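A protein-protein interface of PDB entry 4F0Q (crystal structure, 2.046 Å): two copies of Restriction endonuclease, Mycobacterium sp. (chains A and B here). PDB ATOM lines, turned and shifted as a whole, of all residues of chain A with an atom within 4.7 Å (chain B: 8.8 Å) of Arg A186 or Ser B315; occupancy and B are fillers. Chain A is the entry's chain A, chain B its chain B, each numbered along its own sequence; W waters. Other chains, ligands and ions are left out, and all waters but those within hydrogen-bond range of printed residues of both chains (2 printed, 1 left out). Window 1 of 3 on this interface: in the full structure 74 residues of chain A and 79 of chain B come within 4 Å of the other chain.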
ATOM      1  N   ARG A 113      26.150 -29.805 -10.441  1.00  0.00           N
ATOM      2  CA  ARG A 113      27.257 -28.893 -10.182  1.00  0.00           C
ATOM      3  C   ARG A 113      28.521 -29.703  -9.934  1.00  0.00           C
ATOM      4  O   ARG A 113      28.613 -30.433  -8.947  1.00  0.00           O
ATOM      5  CB  ARG A 113      26.951 -28.015  -8.968  1.00  0.00           C
ATOM      6  CG  ARG A 113      28.079 -27.073  -8.575  1.00  0.00           C
ATOM      7  CD  ARG A 113      28.294 -25.992  -9.623  1.00  0.00           C
ATOM      8  NE  ARG A 113      27.075 -25.229  -9.878  1.00  0.00           N
ATOM      9  CZ  ARG A 113      26.670 -24.195  -9.147  1.00  0.00           C
ATOM     10  NH1 ARG A 113      27.387 -23.793  -8.106  1.00  0.00           N
ATOM     11  NH2 ARG A 113      25.547 -23.562  -9.456  1.00  0.00           N
ATOM     12  N   ILE A 184      27.920 -29.260 -20.875  1.00  0.00           N
ATOM     13  CA  ILE A 184      28.488 -28.181 -20.082  1.00  0.00           C
ATOM     14  C   ILE A 184      27.701 -26.901 -20.335  1.00  0.00           C
ATOM     15  O   ILE A 184      27.922 -26.208 -21.330  1.00  0.00           O
ATOM     16  CB  ILE A 184      29.978 -27.951 -20.403  1.00  0.00           C
ATOM     17  CG1 ILE A 184      30.781 -29.222 -20.127  1.00  0.00           C
ATOM     18  CG2 ILE A 184      30.529 -26.792 -19.584  1.00  0.00           C
ATOM     19  CD1 ILE A 184      32.267 -29.064 -20.348  1.00  0.00           C
ATOM     20  N   GLU A 185      26.770 -26.600 -19.437  1.00  0.00           N
ATOM     21  CA  GLU A 185      25.942 -25.410 -19.574  1.00  0.00           C
ATOM     22  C   GLU A 185      26.714 -24.166 -19.161  1.00  0.00           C
ATOM     23  O   GLU A 185      26.580 -23.107 -19.779  1.00  0.00           O
ATOM     24  CB  GLU A 185      24.662 -25.535 -18.748  1.00  0.00           C
ATOM     25  CG  GLU A 185      23.715 -24.357 -18.910  1.00  0.00           C
ATOM     26  CD  GLU A 185      22.472 -24.485 -18.055  1.00  0.00           C
ATOM     27  OE1 GLU A 185      22.508 -25.236 -17.057  1.00  0.00           O
ATOM     28  OE2 GLU A 185      21.456 -23.839 -18.386  1.00  0.00           O
ATOM     29  N   ARG A 186      27.525 -24.291 -18.118  1.00  0.00           N
ATOM     30  CA  ARG A 186      28.348 -23.167 -17.683  1.00  0.00           C
ATOM     31  C   ARG A 186      29.680 -23.634 -17.101  1.00  0.00           C
ATOM     32  O   ARG A 186      29.768 -24.710 -16.517  1.00  0.00           O
ATOM     33  CB  ARG A 186      27.588 -22.299 -16.676  1.00  0.00           C
ATOM     34  CG  ARG A 186      28.216 -20.936 -16.429  1.00  0.00           C
ATOM     35  CD  ARG A 186      27.272 -20.005 -15.681  1.00  0.00           C
ATOM     36  NE  ARG A 186      26.962 -20.491 -14.340  1.00  0.00           N
ATOM     37  CZ  ARG A 186      26.273 -19.800 -13.437  1.00  0.00           C
ATOM     38  NH1 ARG A 186      25.823 -18.588 -13.730  1.00  0.00           N
ATOM     39  NH2 ARG A 186      26.036 -20.320 -12.239  1.00  0.00           N
ATOM     40  N   LEU A 187      30.719 -22.827 -17.285  1.00  0.00           N
ATOM     41  CA  LEU A 187      32.029 -23.111 -16.710  1.00  0.00           C
ATOM     42  C   LEU A 187      32.626 -21.816 -16.179  1.00  0.00           C
ATOM     43  O   LEU A 187      32.911 -20.897 -16.945  1.00  0.00           O
ATOM     44  CB  LEU A 187      32.955 -23.745 -17.753  1.00  0.00           C
ATOM     45  CG  LEU A 187      34.270 -24.366 -17.262  1.00  0.00           C
ATOM     46  CD1 LEU A 187      34.676 -25.522 -18.162  1.00  0.00           C
ATOM     47  CD2 LEU A 187      35.393 -23.338 -17.194  1.00  0.00           C
ATOM     48  N   GLU A 188      32.820 -21.745 -14.866  1.00  0.00           N
ATOM     49  CA  GLU A 188      33.293 -20.516 -14.241  1.00  0.00           C
ATOM     50  C   GLU A 188      34.456 -20.725 -13.276  1.00  0.00           C
ATOM     51  O   GLU A 188      34.734 -21.844 -12.846  1.00  0.00           O
ATOM     52  CB  GLU A 188      32.138 -19.801 -13.534  1.00  0.00           C
ATOM     53  CG  GLU A 188      31.317 -20.694 -12.624  1.00  0.00           C
ATOM     54  CD  GLU A 188      30.032 -20.033 -12.166  1.00  0.00           C
ATOM     55  OE1 GLU A 188      29.161 -20.740 -11.616  1.00  0.00           O
ATOM     56  OE2 GLU A 188      29.892 -18.806 -12.356  1.00  0.00           O
ATOM     57  N   SER A 205      34.348 -24.454 -11.661  1.00  0.00           N
ATOM     58  CA  SER A 205      33.022 -24.902 -11.259  1.00  0.00           C
ATOM     59  C   SER A 205      32.118 -24.970 -12.484  1.00  0.00           C
ATOM     60  O   SER A 205      32.010 -24.005 -13.240  1.00  0.00           O
ATOM     61  CB  SER A 205      32.429 -23.957 -10.213  1.00  0.00           C
ATOM     62  OG  SER A 205      31.162 -24.411  -9.772  1.00  0.00           O
ATOM     63  N   LEU A 206      31.471 -26.114 -12.677  1.00  0.00           N
ATOM     64  CA  LEU A 206      30.697 -26.355 -13.890  1.00  0.00           C
ATOM     65  C   LEU A 206      29.222 -26.652 -13.623  1.00  0.00           C
ATOM     66  O   LEU A 206      28.884 -27.515 -12.811  1.00  0.00           O
ATOM     67  CB  LEU A 206      31.313 -27.500 -14.705  1.00  0.00           C
ATOM     68  CG  LEU A 206      32.591 -27.245 -15.514  1.00  0.00           C
ATOM     69  CD1 LEU A 206      33.820 -27.130 -14.625  1.00  0.00           C
ATOM     70  CD2 LEU A 206      32.786 -28.338 -16.556  1.00  0.00           C
ATOM     71  N   ASP A 207      28.356 -25.916 -14.314  1.00  0.00           N
ATOM     72  CA  ASP A 207      26.935 -26.225 -14.366  1.00  0.00           C
ATOM     73  C   ASP A 207      26.682 -27.169 -15.530  1.00  0.00           C
ATOM     74  O   ASP A 207      26.846 -26.792 -16.696  1.00  0.00           O
ATOM     75  CB  ASP A 207      26.105 -24.954 -14.550  1.00  0.00           C
ATOM     76  CG  ASP A 207      26.048 -24.106 -13.298  1.00  0.00           C
ATOM     77  OD1 ASP A 207      26.063 -24.678 -12.188  1.00  0.00           O
ATOM     78  OD2 ASP A 207      25.981 -22.866 -13.426  1.00  0.00           O
ATOM     79  N   GLU A 314      23.659 -17.940  -5.706  1.00  0.00           N
ATOM     80  CA  GLU A 314      24.107 -19.279  -6.076  1.00  0.00           C
ATOM     81  C   GLU A 314      23.383 -19.759  -7.329  1.00  0.00           C
ATOM     82  O   GLU A 314      23.905 -20.577  -8.089  1.00  0.00           O
ATOM     83  CB  GLU A 314      23.888 -20.262  -4.919  1.00  0.00           C
ATOM     84  CG  GLU A 314      24.396 -21.679  -5.179  1.00  0.00           C
ATOM     85  CD  GLU A 314      25.912 -21.780  -5.184  1.00  0.00           C
ATOM     86  OE1 GLU A 314      26.577 -20.822  -4.737  1.00  0.00           O
ATOM     87  OE2 GLU A 314      26.441 -22.816  -5.640  1.00  0.00           O
ATOM     88  N   GLY A 316      22.635 -17.781  -9.714  1.00  0.00           N
ATOM     89  CA  GLY A 316      22.948 -16.788 -10.725  1.00  0.00           C
ATOM     90  C   GLY A 316      22.118 -15.524 -10.604  1.00  0.00           C
ATOM     91  O   GLY A 316      22.367 -14.542 -11.308  1.00  0.00           O
ATOM     92  N   ARG A 318      20.944 -12.054  -9.540  1.00  0.00           N
ATOM     93  CA  ARG A 318      21.642 -10.864  -9.067  1.00  0.00           C
ATOM     94  C   ARG A 318      20.897 -10.201  -7.917  1.00  0.00           C
ATOM     95  O   ARG A 318      19.943  -9.460  -8.124  1.00  0.00           O
ATOM     96  CB  ARG A 318      21.890  -9.883 -10.215  1.00  0.00           C
ATOM     97  CG  ARG A 318      22.724 -10.485 -11.342  1.00  0.00           C
ATOM     98  CD  ARG A 318      23.182  -9.432 -12.337  1.00  0.00           C
ATOM     99  NE  ARG A 318      23.766  -8.263 -11.686  1.00  0.00           N
ATOM    100  CZ  ARG A 318      25.042  -8.153 -11.328  1.00  0.00           C
ATOM    101  NH1 ARG A 318      25.887  -9.152 -11.552  1.00  0.00           N
ATOM    102  NH2 ARG A 318      25.467  -7.041 -10.741  1.00  0.00           N
ATOM    103  N   GLY A 342      16.276 -10.577 -15.242  1.00  0.00           N
ATOM    104  CA  GLY A 342      16.515 -10.239 -16.633  1.00  0.00           C
ATOM    105  C   GLY A 342      18.000 -10.176 -16.922  1.00  0.00           C
ATOM    106  O   GLY A 342      18.774 -10.987 -16.413  1.00  0.00           O
ATOM    107  N   HIS B 111      27.423  -2.234 -12.441  1.00  0.00           N
ATOM    108  CA  HIS B 111      27.655  -3.527 -13.070  1.00  0.00           C
ATOM    109  C   HIS B 111      28.309  -3.357 -14.435  1.00  0.00           C
ATOM    110  O   HIS B 111      27.823  -2.601 -15.275  1.00  0.00           O
ATOM    111  CB  HIS B 111      26.339  -4.296 -13.209  1.00  0.00           C
ATOM    112  CG  HIS B 111      26.505  -5.687 -13.738  1.00  0.00           C
ATOM    113  ND1 HIS B 111      25.471  -6.394 -14.314  1.00  0.00           N
ATOM    114  CD2 HIS B 111      27.584  -6.505 -13.774  1.00  0.00           C
ATOM    115  CE1 HIS B 111      25.905  -7.585 -14.685  1.00  0.00           C
ATOM    116  NE2 HIS B 111      27.184  -7.678 -14.369  1.00  0.00           N
ATOM    117  N   ARG B 113      30.039  -5.680 -17.698  1.00  0.00           N
ATOM    118  CA  ARG B 113      30.416  -6.938 -18.329  1.00  0.00           C
ATOM    119  C   ARG B 113      31.647  -6.731 -19.203  1.00  0.00           C
ATOM    120  O   ARG B 113      31.612  -5.963 -20.164  1.00  0.00           O
ATOM    121  CB  ARG B 113      29.263  -7.509 -19.155  1.00  0.00           C
ATOM    122  CG  ARG B 113      28.055  -7.925 -18.333  1.00  0.00           C
ATOM    123  CD  ARG B 113      27.370  -9.136 -18.946  1.00  0.00           C
ATOM    124  NE  ARG B 113      28.252 -10.301 -18.957  1.00  0.00           N
ATOM    125  CZ  ARG B 113      27.931 -11.480 -19.477  1.00  0.00           C
ATOM    126  NH1 ARG B 113      26.743 -11.659 -20.039  1.00  0.00           N
ATOM    127  NH2 ARG B 113      28.798 -12.482 -19.440  1.00  0.00           N
ATOM    128  N   GLU B 185      33.322  -9.861  -9.661  1.00  0.00           N
ATOM    129  CA  GLU B 185      32.232 -10.566  -8.998  1.00  0.00           C
ATOM    130  C   GLU B 185      32.052 -11.969  -9.569  1.00  0.00           C
ATOM    131  O   GLU B 185      31.732 -12.908  -8.840  1.00  0.00           O
ATOM    132  CB  GLU B 185      30.928  -9.774  -9.122  1.00  0.00           C
ATOM    133  CG  GLU B 185      29.755 -10.387  -8.377  1.00  0.00           C
ATOM    134  CD  GLU B 185      28.512  -9.524  -8.441  1.00  0.00           C
ATOM    135  OE1 GLU B 185      28.563  -8.453  -9.082  1.00  0.00           O
ATOM    136  OE2 GLU B 185      27.483  -9.915  -7.850  1.00  0.00           O
ATOM    137  N   ARG B 186      32.261 -12.109 -10.873  1.00  0.00           N
ATOM    138  CA  ARG B 186      32.171 -13.421 -11.508  1.00  0.00           C
ATOM    139  C   ARG B 186      33.139 -13.531 -12.681  1.00  0.00           C
ATOM    140  O   ARG B 186      33.420 -12.547 -13.356  1.00  0.00           O
ATOM    141  CB  ARG B 186      30.735 -13.702 -11.964  1.00  0.00           C
ATOM    142  CG  ARG B 186      30.473 -15.151 -12.353  1.00  0.00           C
ATOM    143  CD  ARG B 186      28.997 -15.403 -12.628  1.00  0.00           C
ATOM    144  NE  ARG B 186      28.504 -14.616 -13.755  1.00  0.00           N
ATOM    145  CZ  ARG B 186      27.276 -14.713 -14.255  1.00  0.00           C
ATOM    146  NH1 ARG B 186      26.410 -15.568 -13.728  1.00  0.00           N
ATOM    147  NH2 ARG B 186      26.912 -13.958 -15.282  1.00  0.00           N
ATOM    148  N   LEU B 187      33.658 -14.734 -12.906  1.00  0.00           N
ATOM    149  CA  LEU B 187      34.546 -14.988 -14.033  1.00  0.00           C
ATOM    150  C   LEU B 187      34.246 -16.370 -14.601  1.00  0.00           C
ATOM    151  O   LEU B 187      34.408 -17.379 -13.916  1.00  0.00           O
ATOM    152  CB  LEU B 187      36.014 -14.884 -13.602  1.00  0.00           C
ATOM    153  CG  LEU B 187      37.090 -14.760 -14.689  1.00  0.00           C
ATOM    154  CD1 LEU B 187      38.319 -14.053 -14.138  1.00  0.00           C
ATOM    155  CD2 LEU B 187      37.484 -16.116 -15.262  1.00  0.00           C
ATOM    156  N   GLU B 188      33.810 -16.412 -15.855  1.00  0.00           N
ATOM    157  CA  GLU B 188      33.431 -17.675 -16.475  1.00  0.00           C
ATOM    158  C   GLU B 188      34.009 -17.856 -17.875  1.00  0.00           C
ATOM    159  O   GLU B 188      34.596 -16.937 -18.445  1.00  0.00           O
ATOM    160  CB  GLU B 188      31.908 -17.826 -16.503  1.00  0.00           C
ATOM    161  CG  GLU B 188      31.177 -16.728 -17.251  1.00  0.00           C
ATOM    162  CD  GLU B 188      29.674 -16.816 -17.074  1.00  0.00           C
ATOM    163  OE1 GLU B 188      28.939 -16.271 -17.923  1.00  0.00           O
ATOM    164  OE2 GLU B 188      29.231 -17.427 -16.080  1.00  0.00           O
ATOM    165  N   HIS B 189      33.838 -19.057 -18.415  1.00  0.00           N
ATOM    166  CA  HIS B 189      34.324 -19.387 -19.745  1.00  0.00           C
ATOM    167  C   HIS B 189      33.304 -18.943 -20.784  1.00  0.00           C
ATOM    168  O   HIS B 189      32.099 -19.071 -20.572  1.00  0.00           O
ATOM    169  CB  HIS B 189      34.561 -20.895 -19.848  1.00  0.00           C
ATOM    170  CG  HIS B 189      35.248 -21.320 -21.109  1.00  0.00           C
ATOM    171  ND1 HIS B 189      34.560 -21.732 -22.230  1.00  0.00           N
ATOM    172  CD2 HIS B 189      36.562 -21.410 -21.422  1.00  0.00           C
ATOM    173  CE1 HIS B 189      35.420 -22.050 -23.180  1.00  0.00           C
ATOM    174  NE2 HIS B 189      36.642 -21.864 -22.715  1.00  0.00           N
ATOM    175  N   VAL B 190      33.784 -18.413 -21.902  1.00  0.00           N
ATOM    176  CA  VAL B 190      32.892 -18.004 -22.980  1.00  0.00           C
ATOM    177  C   VAL B 190      33.460 -18.439 -24.329  1.00  0.00           C
ATOM    178  O   VAL B 190      34.670 -18.561 -24.490  1.00  0.00           O
ATOM    179  CB  VAL B 190      32.636 -16.473 -22.958  1.00  0.00           C
ATOM    180  CG1 VAL B 190      33.886 -15.707 -23.359  1.00  0.00           C
ATOM    181  CG2 VAL B 190      31.465 -16.101 -23.859  1.00  0.00           C
ATOM    182  N   ASP B 207      31.955 -10.576 -14.854  1.00  0.00           N
ATOM    183  CA  ASP B 207      30.969  -9.703 -14.238  1.00  0.00           C
ATOM    184  C   ASP B 207      31.655  -8.901 -13.139  1.00  0.00           C
ATOM    185  O   ASP B 207      32.134  -9.464 -12.150  1.00  0.00           O
ATOM    186  CB  ASP B 207      29.810 -10.511 -13.658  1.00  0.00           C
ATOM    187  CG  ASP B 207      28.990 -11.201 -14.728  1.00  0.00           C
ATOM    188  OD1 ASP B 207      28.082 -10.555 -15.291  1.00  0.00           O
ATOM    189  OD2 ASP B 207      29.254 -12.390 -15.007  1.00  0.00           O
ATOM    190  N   ALA B 309      14.323 -16.228 -23.226  1.00  0.00           N
ATOM    191  CA  ALA B 309      15.105 -17.286 -22.598  1.00  0.00           C
ATOM    192  C   ALA B 309      16.569 -16.879 -22.492  1.00  0.00           C
ATOM    193  O   ALA B 309      17.216 -17.117 -21.474  1.00  0.00           O
ATOM    194  CB  ALA B 309      14.969 -18.584 -23.375  1.00  0.00           C
ATOM    195  N   GLU B 310      17.085 -16.253 -23.545  1.00  0.00           N
ATOM    196  CA  GLU B 310      18.484 -15.836 -23.571  1.00  0.00           C
ATOM    197  C   GLU B 310      18.756 -14.682 -22.605  1.00  0.00           C
ATOM    198  O   GLU B 310      19.805 -14.633 -21.962  1.00  0.00           O
ATOM    199  CB  GLU B 310      18.903 -15.454 -24.995  1.00  0.00           C
ATOM    200  CG  GLU B 310      20.378 -15.104 -25.151  1.00  0.00           C
ATOM    201  CD  GLU B 310      21.284 -16.323 -25.158  1.00  0.00           C
ATOM    202  OE1 GLU B 310      20.773 -17.457 -25.039  1.00  0.00           O
ATOM    203  OE2 GLU B 310      22.513 -16.144 -25.288  1.00  0.00           O
ATOM    204  N   VAL B 311      17.805 -13.759 -22.506  1.00  0.00           N
ATOM    205  CA  VAL B 311      17.924 -12.614 -21.610  1.00  0.00           C
ATOM    206  C   VAL B 311      17.893 -13.051 -20.148  1.00  0.00           C
ATOM    207  O   VAL B 311      18.692 -12.587 -19.332  1.00  0.00           O
ATOM    208  CB  VAL B 311      16.801 -11.581 -21.864  1.00  0.00           C
ATOM    209  CG1 VAL B 311      16.764 -10.538 -20.757  1.00  0.00           C
ATOM    210  CG2 VAL B 311      16.983 -10.919 -23.222  1.00  0.00           C
ATOM    211  N   PHE B 312      16.974 -13.955 -19.822  1.00  0.00           N
ATOM    212  CA  PHE B 312      16.820 -14.420 -18.446  1.00  0.00           C
ATOM    213  C   PHE B 312      17.955 -15.332 -17.977  1.00  0.00           C
ATOM    214  O   PHE B 312      18.080 -15.605 -16.784  1.00  0.00           O
ATOM    215  CB  PHE B 312      15.473 -15.122 -18.267  1.00  0.00           C
ATOM    216  CG  PHE B 312      14.320 -14.178 -18.083  1.00  0.00           C
ATOM    217  CD1 PHE B 312      14.391 -13.150 -17.158  1.00  0.00           C
ATOM    218  CD2 PHE B 312      13.169 -14.312 -18.839  1.00  0.00           C
ATOM    219  CE1 PHE B 312      13.334 -12.279 -16.986  1.00  0.00           C
ATOM    220  CE2 PHE B 312      12.108 -13.442 -18.672  1.00  0.00           C
ATOM    221  CZ  PHE B 312      12.192 -12.425 -17.745  1.00  0.00           C
ATOM    222  N   ARG B 313      18.781 -15.795 -18.910  1.00  0.00           N
ATOM    223  CA  ARG B 313      19.863 -16.718 -18.572  1.00  0.00           C
ATOM    224  C   ARG B 313      21.235 -16.051 -18.516  1.00  0.00           C
ATOM    225  O   ARG B 313      22.228 -16.701 -18.190  1.00  0.00           O
ATOM    226  CB  ARG B 313      19.900 -17.890 -19.555  1.00  0.00           C
ATOM    227  CG  ARG B 313      18.774 -18.895 -19.382  1.00  0.00           C
ATOM    228  CD  ARG B 313      18.881 -20.000 -20.419  1.00  0.00           C
ATOM    229  NE  ARG B 313      20.112 -20.771 -20.266  1.00  0.00           N
ATOM    230  CZ  ARG B 313      20.729 -21.403 -21.259  1.00  0.00           C
ATOM    231  NH1 ARG B 313      20.238 -21.350 -22.489  1.00  0.00           N
ATOM    232  NH2 ARG B 313      21.844 -22.080 -21.024  1.00  0.00           N
ATOM    233  N   GLU B 314      21.291 -14.762 -18.838  1.00  0.00           N
ATOM    234  CA  GLU B 314      22.556 -14.030 -18.833  1.00  0.00           C
ATOM    235  C   GLU B 314      23.192 -14.016 -17.447  1.00  0.00           C
ATOM    236  O   GLU B 314      24.382 -14.295 -17.296  1.00  0.00           O
ATOM    237  CB  GLU B 314      22.361 -12.595 -19.327  1.00  0.00           C
ATOM    238  CG  GLU B 314      23.564 -11.701 -19.064  1.00  0.00           C
ATOM    239  CD  GLU B 314      23.413 -10.315 -19.657  1.00  0.00           C
ATOM    240  OE1 GLU B 314      23.628  -9.328 -18.922  1.00  0.00           O
ATOM    241  OE2 GLU B 314      23.092 -10.212 -20.859  1.00  0.00           O
ATOM    242  N   SER B 315      22.387 -13.693 -16.441  1.00  0.00           N
ATOM    243  CA  SER B 315      22.855 -13.650 -15.062  1.00  0.00           C
ATOM    244  C   SER B 315      23.208 -15.044 -14.555  1.00  0.00           C
ATOM    245  O   SER B 315      23.991 -15.196 -13.618  1.00  0.00           O
ATOM    246  CB  SER B 315      21.793 -13.014 -14.161  1.00  0.00           C
ATOM    247  OG  SER B 315      20.560 -13.705 -14.263  1.00  0.00           O
ATOM    248  N   GLY B 316      22.627 -16.060 -15.183  1.00  0.00           N
ATOM    249  CA  GLY B 316      22.859 -17.435 -14.788  1.00  0.00           C
ATOM    250  C   GLY B 316      21.622 -18.040 -14.157  1.00  0.00           C
ATOM    251  O   GLY B 316      21.663 -19.150 -13.626  1.00  0.00           O
ATOM    252  N   ALA B 317      20.518 -17.301 -14.216  1.00  0.00           N
ATOM    253  CA  ALA B 317      19.251 -17.761 -13.664  1.00  0.00           C
ATOM    254  C   ALA B 317      18.744 -18.991 -14.405  1.00  0.00           C
ATOM    255  O   ALA B 317      18.963 -19.141 -15.606  1.00  0.00           O
ATOM    256  CB  ALA B 317      18.216 -16.650 -13.705  1.00  0.00           C
ATOM    257  N   ARG B 318      18.061 -19.868 -13.678  1.00  0.00           N
ATOM    258  CA  ARG B 318      17.589 -21.128 -14.235  1.00  0.00           C
ATOM    259  C   ARG B 318      16.258 -20.945 -14.953  1.00  0.00           C
ATOM    260  O   ARG B 318      15.194 -21.078 -14.351  1.00  0.00           O
ATOM    261  CB  ARG B 318      17.455 -22.169 -13.124  1.00  0.00           C
ATOM    262  CG  ARG B 318      18.548 -22.068 -12.074  1.00  0.00           C
ATOM    263  CD  ARG B 318      19.275 -23.385 -11.876  1.00  0.00           C
ATOM    264  NE  ARG B 318      20.528 -23.196 -11.150  1.00  0.00           N
ATOM    265  CZ  ARG B 318      21.337 -24.181 -10.778  1.00  0.00           C
ATOM    266  NH1 ARG B 318      21.026 -25.439 -11.055  1.00  0.00           N
ATOM    267  NH2 ARG B 318      22.458 -23.908 -10.123  1.00  0.00           N
ATOM    268  N   TYR B 319      16.326 -20.637 -16.244  1.00  0.00           N
ATOM    269  CA  TYR B 319      15.127 -20.441 -17.046  1.00  0.00           C
ATOM    270  C   TYR B 319      14.727 -21.735 -17.744  1.00  0.00           C
ATOM    271  O   TYR B 319      15.526 -22.343 -18.455  1.00  0.00           O
ATOM    272  CB  TYR B 319      15.347 -19.331 -18.079  1.00  0.00           C
ATOM    273  CG  TYR B 319      14.103 -18.944 -18.850  1.00  0.00           C
ATOM    274  CD1 TYR B 319      13.262 -17.941 -18.388  1.00  0.00           C
ATOM    275  CD2 TYR B 319      13.774 -19.574 -20.044  1.00  0.00           C
ATOM    276  CE1 TYR B 319      12.126 -17.581 -19.086  1.00  0.00           C
ATOM    277  CE2 TYR B 319      12.639 -19.220 -20.750  1.00  0.00           C
ATOM    278  CZ  TYR B 319      11.819 -18.222 -20.266  1.00  0.00           C
ATOM    279  OH  TYR B 319      10.688 -17.862 -20.963  1.00  0.00           O
ATOM    280  N   ILE B 339      11.114 -19.689 -14.226  1.00  0.00           N
ATOM    281  CA  ILE B 339      12.398 -19.369 -13.609  1.00  0.00           C
ATOM    282  C   ILE B 339      12.480 -19.878 -12.173  1.00  0.00           C
ATOM    283  O   ILE B 339      11.847 -19.329 -11.274  1.00  0.00           O
ATOM    284  CB  ILE B 339      12.669 -17.853 -13.611  1.00  0.00           C
ATOM    285  CG1 ILE B 339      12.596 -17.296 -15.033  1.00  0.00           C
ATOM    286  CG2 ILE B 339      14.025 -17.555 -12.990  1.00  0.00           C
ATOM    287  CD1 ILE B 339      12.889 -15.821 -15.132  1.00  0.00           C
ATOM    288  N   MET B 341      14.037 -19.951  -8.806  1.00  0.00           N
ATOM    289  CA  MET B 341      14.879 -18.962  -8.140  1.00  0.00           C
ATOM    290  C   MET B 341      15.438 -19.361  -6.773  1.00  0.00           C
ATOM    291  O   MET B 341      14.707 -19.796  -5.882  1.00  0.00           O
ATOM    292  CB  MET B 341      14.162 -17.611  -8.043  1.00  0.00           C
ATOM    293  CG  MET B 341      13.839 -16.994  -9.394  1.00  0.00           C
ATOM    294  SD  MET B 341      13.735 -15.196  -9.353  1.00  0.00           S
ATOM    295  CE  MET B 341      12.447 -14.958  -8.137  1.00  0.00           C
ATOM    296  N   LEU B 344      17.604 -24.027  -4.928  1.00  0.00           N
ATOM    297  CA  LEU B 344      18.337 -25.162  -5.517  1.00  0.00           C
ATOM    298  C   LEU B 344      18.163 -26.466  -4.740  1.00  0.00           C
ATOM    299  O   LEU B 344      18.546 -27.531  -5.220  1.00  0.00           O
ATOM    300  CB  LEU B 344      19.831 -24.848  -5.683  1.00  0.00           C
ATOM    301  CG  LEU B 344      20.150 -23.640  -6.565  1.00  0.00           C
ATOM    302  CD1 LEU B 344      21.644 -23.557  -6.795  1.00  0.00           C
ATOM    303  CD2 LEU B 344      19.390 -23.744  -7.876  1.00  0.00           C
HETATM  304  O   HOH W   1      17.451 -13.240 -14.546  1.00  0.00           O
HETATM  305  O   HOH W   2      19.840 -21.514 -17.594  1.00  0.00           O
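Of the 23 printed residues of chain B, 13 touch a printed residue of chain A.
Printed residues of chain A that touch a printed residue of chain B: Arg A113, Glu A185, Arg A186, Leu A187, Glu A188, Glu A314, Gly A316, Arg A318 and Gly A342.
Among the printed residues, Asp or Glu carboxylates within 4 Å of a Lys or Arg side-chain nitrogen of the other chain: Glu A185 with Arg B313 (3.2 Å) and Arg A318 with Glu B185 (3.7 Å).
Arg A186 touches Glu B188, and with the chains exchanged Glu A188 touches Arg B186.
Arg A186 touches Gly B316, but with the chains exchanged Gly A316 does not touch Arg B186 (4.7 Å).
Glu A188 touches its own counterpart, Glu B188.
9 positions are printed for both chains.
Of the 20 pairs that touch across the chains among the printed residues, 7 have their exchanged pair printed and touching as well.
Of chain B, only Arg B186 (3.1 Å), Glu B188 (3.3 Å), Ser B315 (3.9 Å) and Gly B316 (3.4 Å) come within 4 Å of Arg A186.
Printed residues of chain A within 4 Å of Ser B315: Arg A186, Gly A316, Arg A318 and Gly A342.
No residue of chain B comes within 4 Å of Asp A207.
Of the printed residues of chain A, His B111 touches Arg A318 (3.4 Å).
Of the printed residues of chain A, His B189 touches Leu A187 (2.5 Å).
Of the printed residues of chain B, Arg A318 touches His B111 (3.4 Å), Glu B185 (3.7 Å) and Ser B315 (3.9 Å).
Printed residues of chain A within 4 Å of Glu B185: Arg A318 (3.7 Å).
OE1 of Glu B185 is in salt-bridge range of NH1 of Arg A318.
The guanidinium group (NH1) of Arg A318 sits at hydrogen-bond distance from a ring nitrogen (NE2) of His B111 (3.4 Å).
The backbone NH of His B189 sits at hydrogen-bond distance from the backbone carbonyl oxygen of Leu A187, at 2.5 Å.
The backbone carbonyl oxygen (O) of Gly A342 sits close to the backbone carbonyl oxygen (O) of Val B311 (3.3 Å).
The guanidinium group (NH2) of Arg A113 sits close to the guanidinium group (NH2) of Arg B318.
The backbone carbonyl oxygen (O) of Ser B315 sits close to the backbone carbonyl oxygen (O) of Gly A316 (2.9 Å).
The side-chain carboxylate of Glu A185 lies within salt-bridge range of the guanidinium group of Arg B313 (3.2 Å).
NH1 of Arg A186 sits close to NH1 of Arg B186, 3.1 Å away.
The guanidinium group of Arg A113 is in salt-bridge range of the side-chain carboxylate of Asp A207 (2.6 Å).
NE of Arg B186 lies within salt-bridge range of OD2 of Asp B207.
The backbone NH of Glu B185 is in hydrogen-bond range of the backbone carbonyl oxygen of Asp B207 (2.8 Å).
The side-chain carboxylate (OE1) of Glu A188 lies within salt-bridge range of the guanidinium group (NH2) of Arg A186 (3.2 Å).
Water W2 lies within hydrogen-bond range of the guanidinium group of Arg B313, the side-chain carboxylate of Glu A185 and the backbone carbonyl oxygen of Ala B317.
Water W1 lies within hydrogen-bond range of the backbone NH of Gly A342 (3.0 Å), the side-chain hydroxyl of Ser B315 (3.2 Å) and the backbone carbonyl oxygen of Phe B312 (3.3 Å).
Among the printed residues, merely in contact across the chains: Arg A186 with Glu B188, Arg A186 with Ser B315, Arg A186 with Gly B316, Leu A187 with Glu B188, Glu A188 with Arg B186, Glu A188 with Leu B187, Glu A188 with Glu B188, Glu A314 with Leu B344, Gly A316 with Gly B316, Arg A318 with Ser B315, Gly A342 with Phe B312 and Gly A342 with Ser B315.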
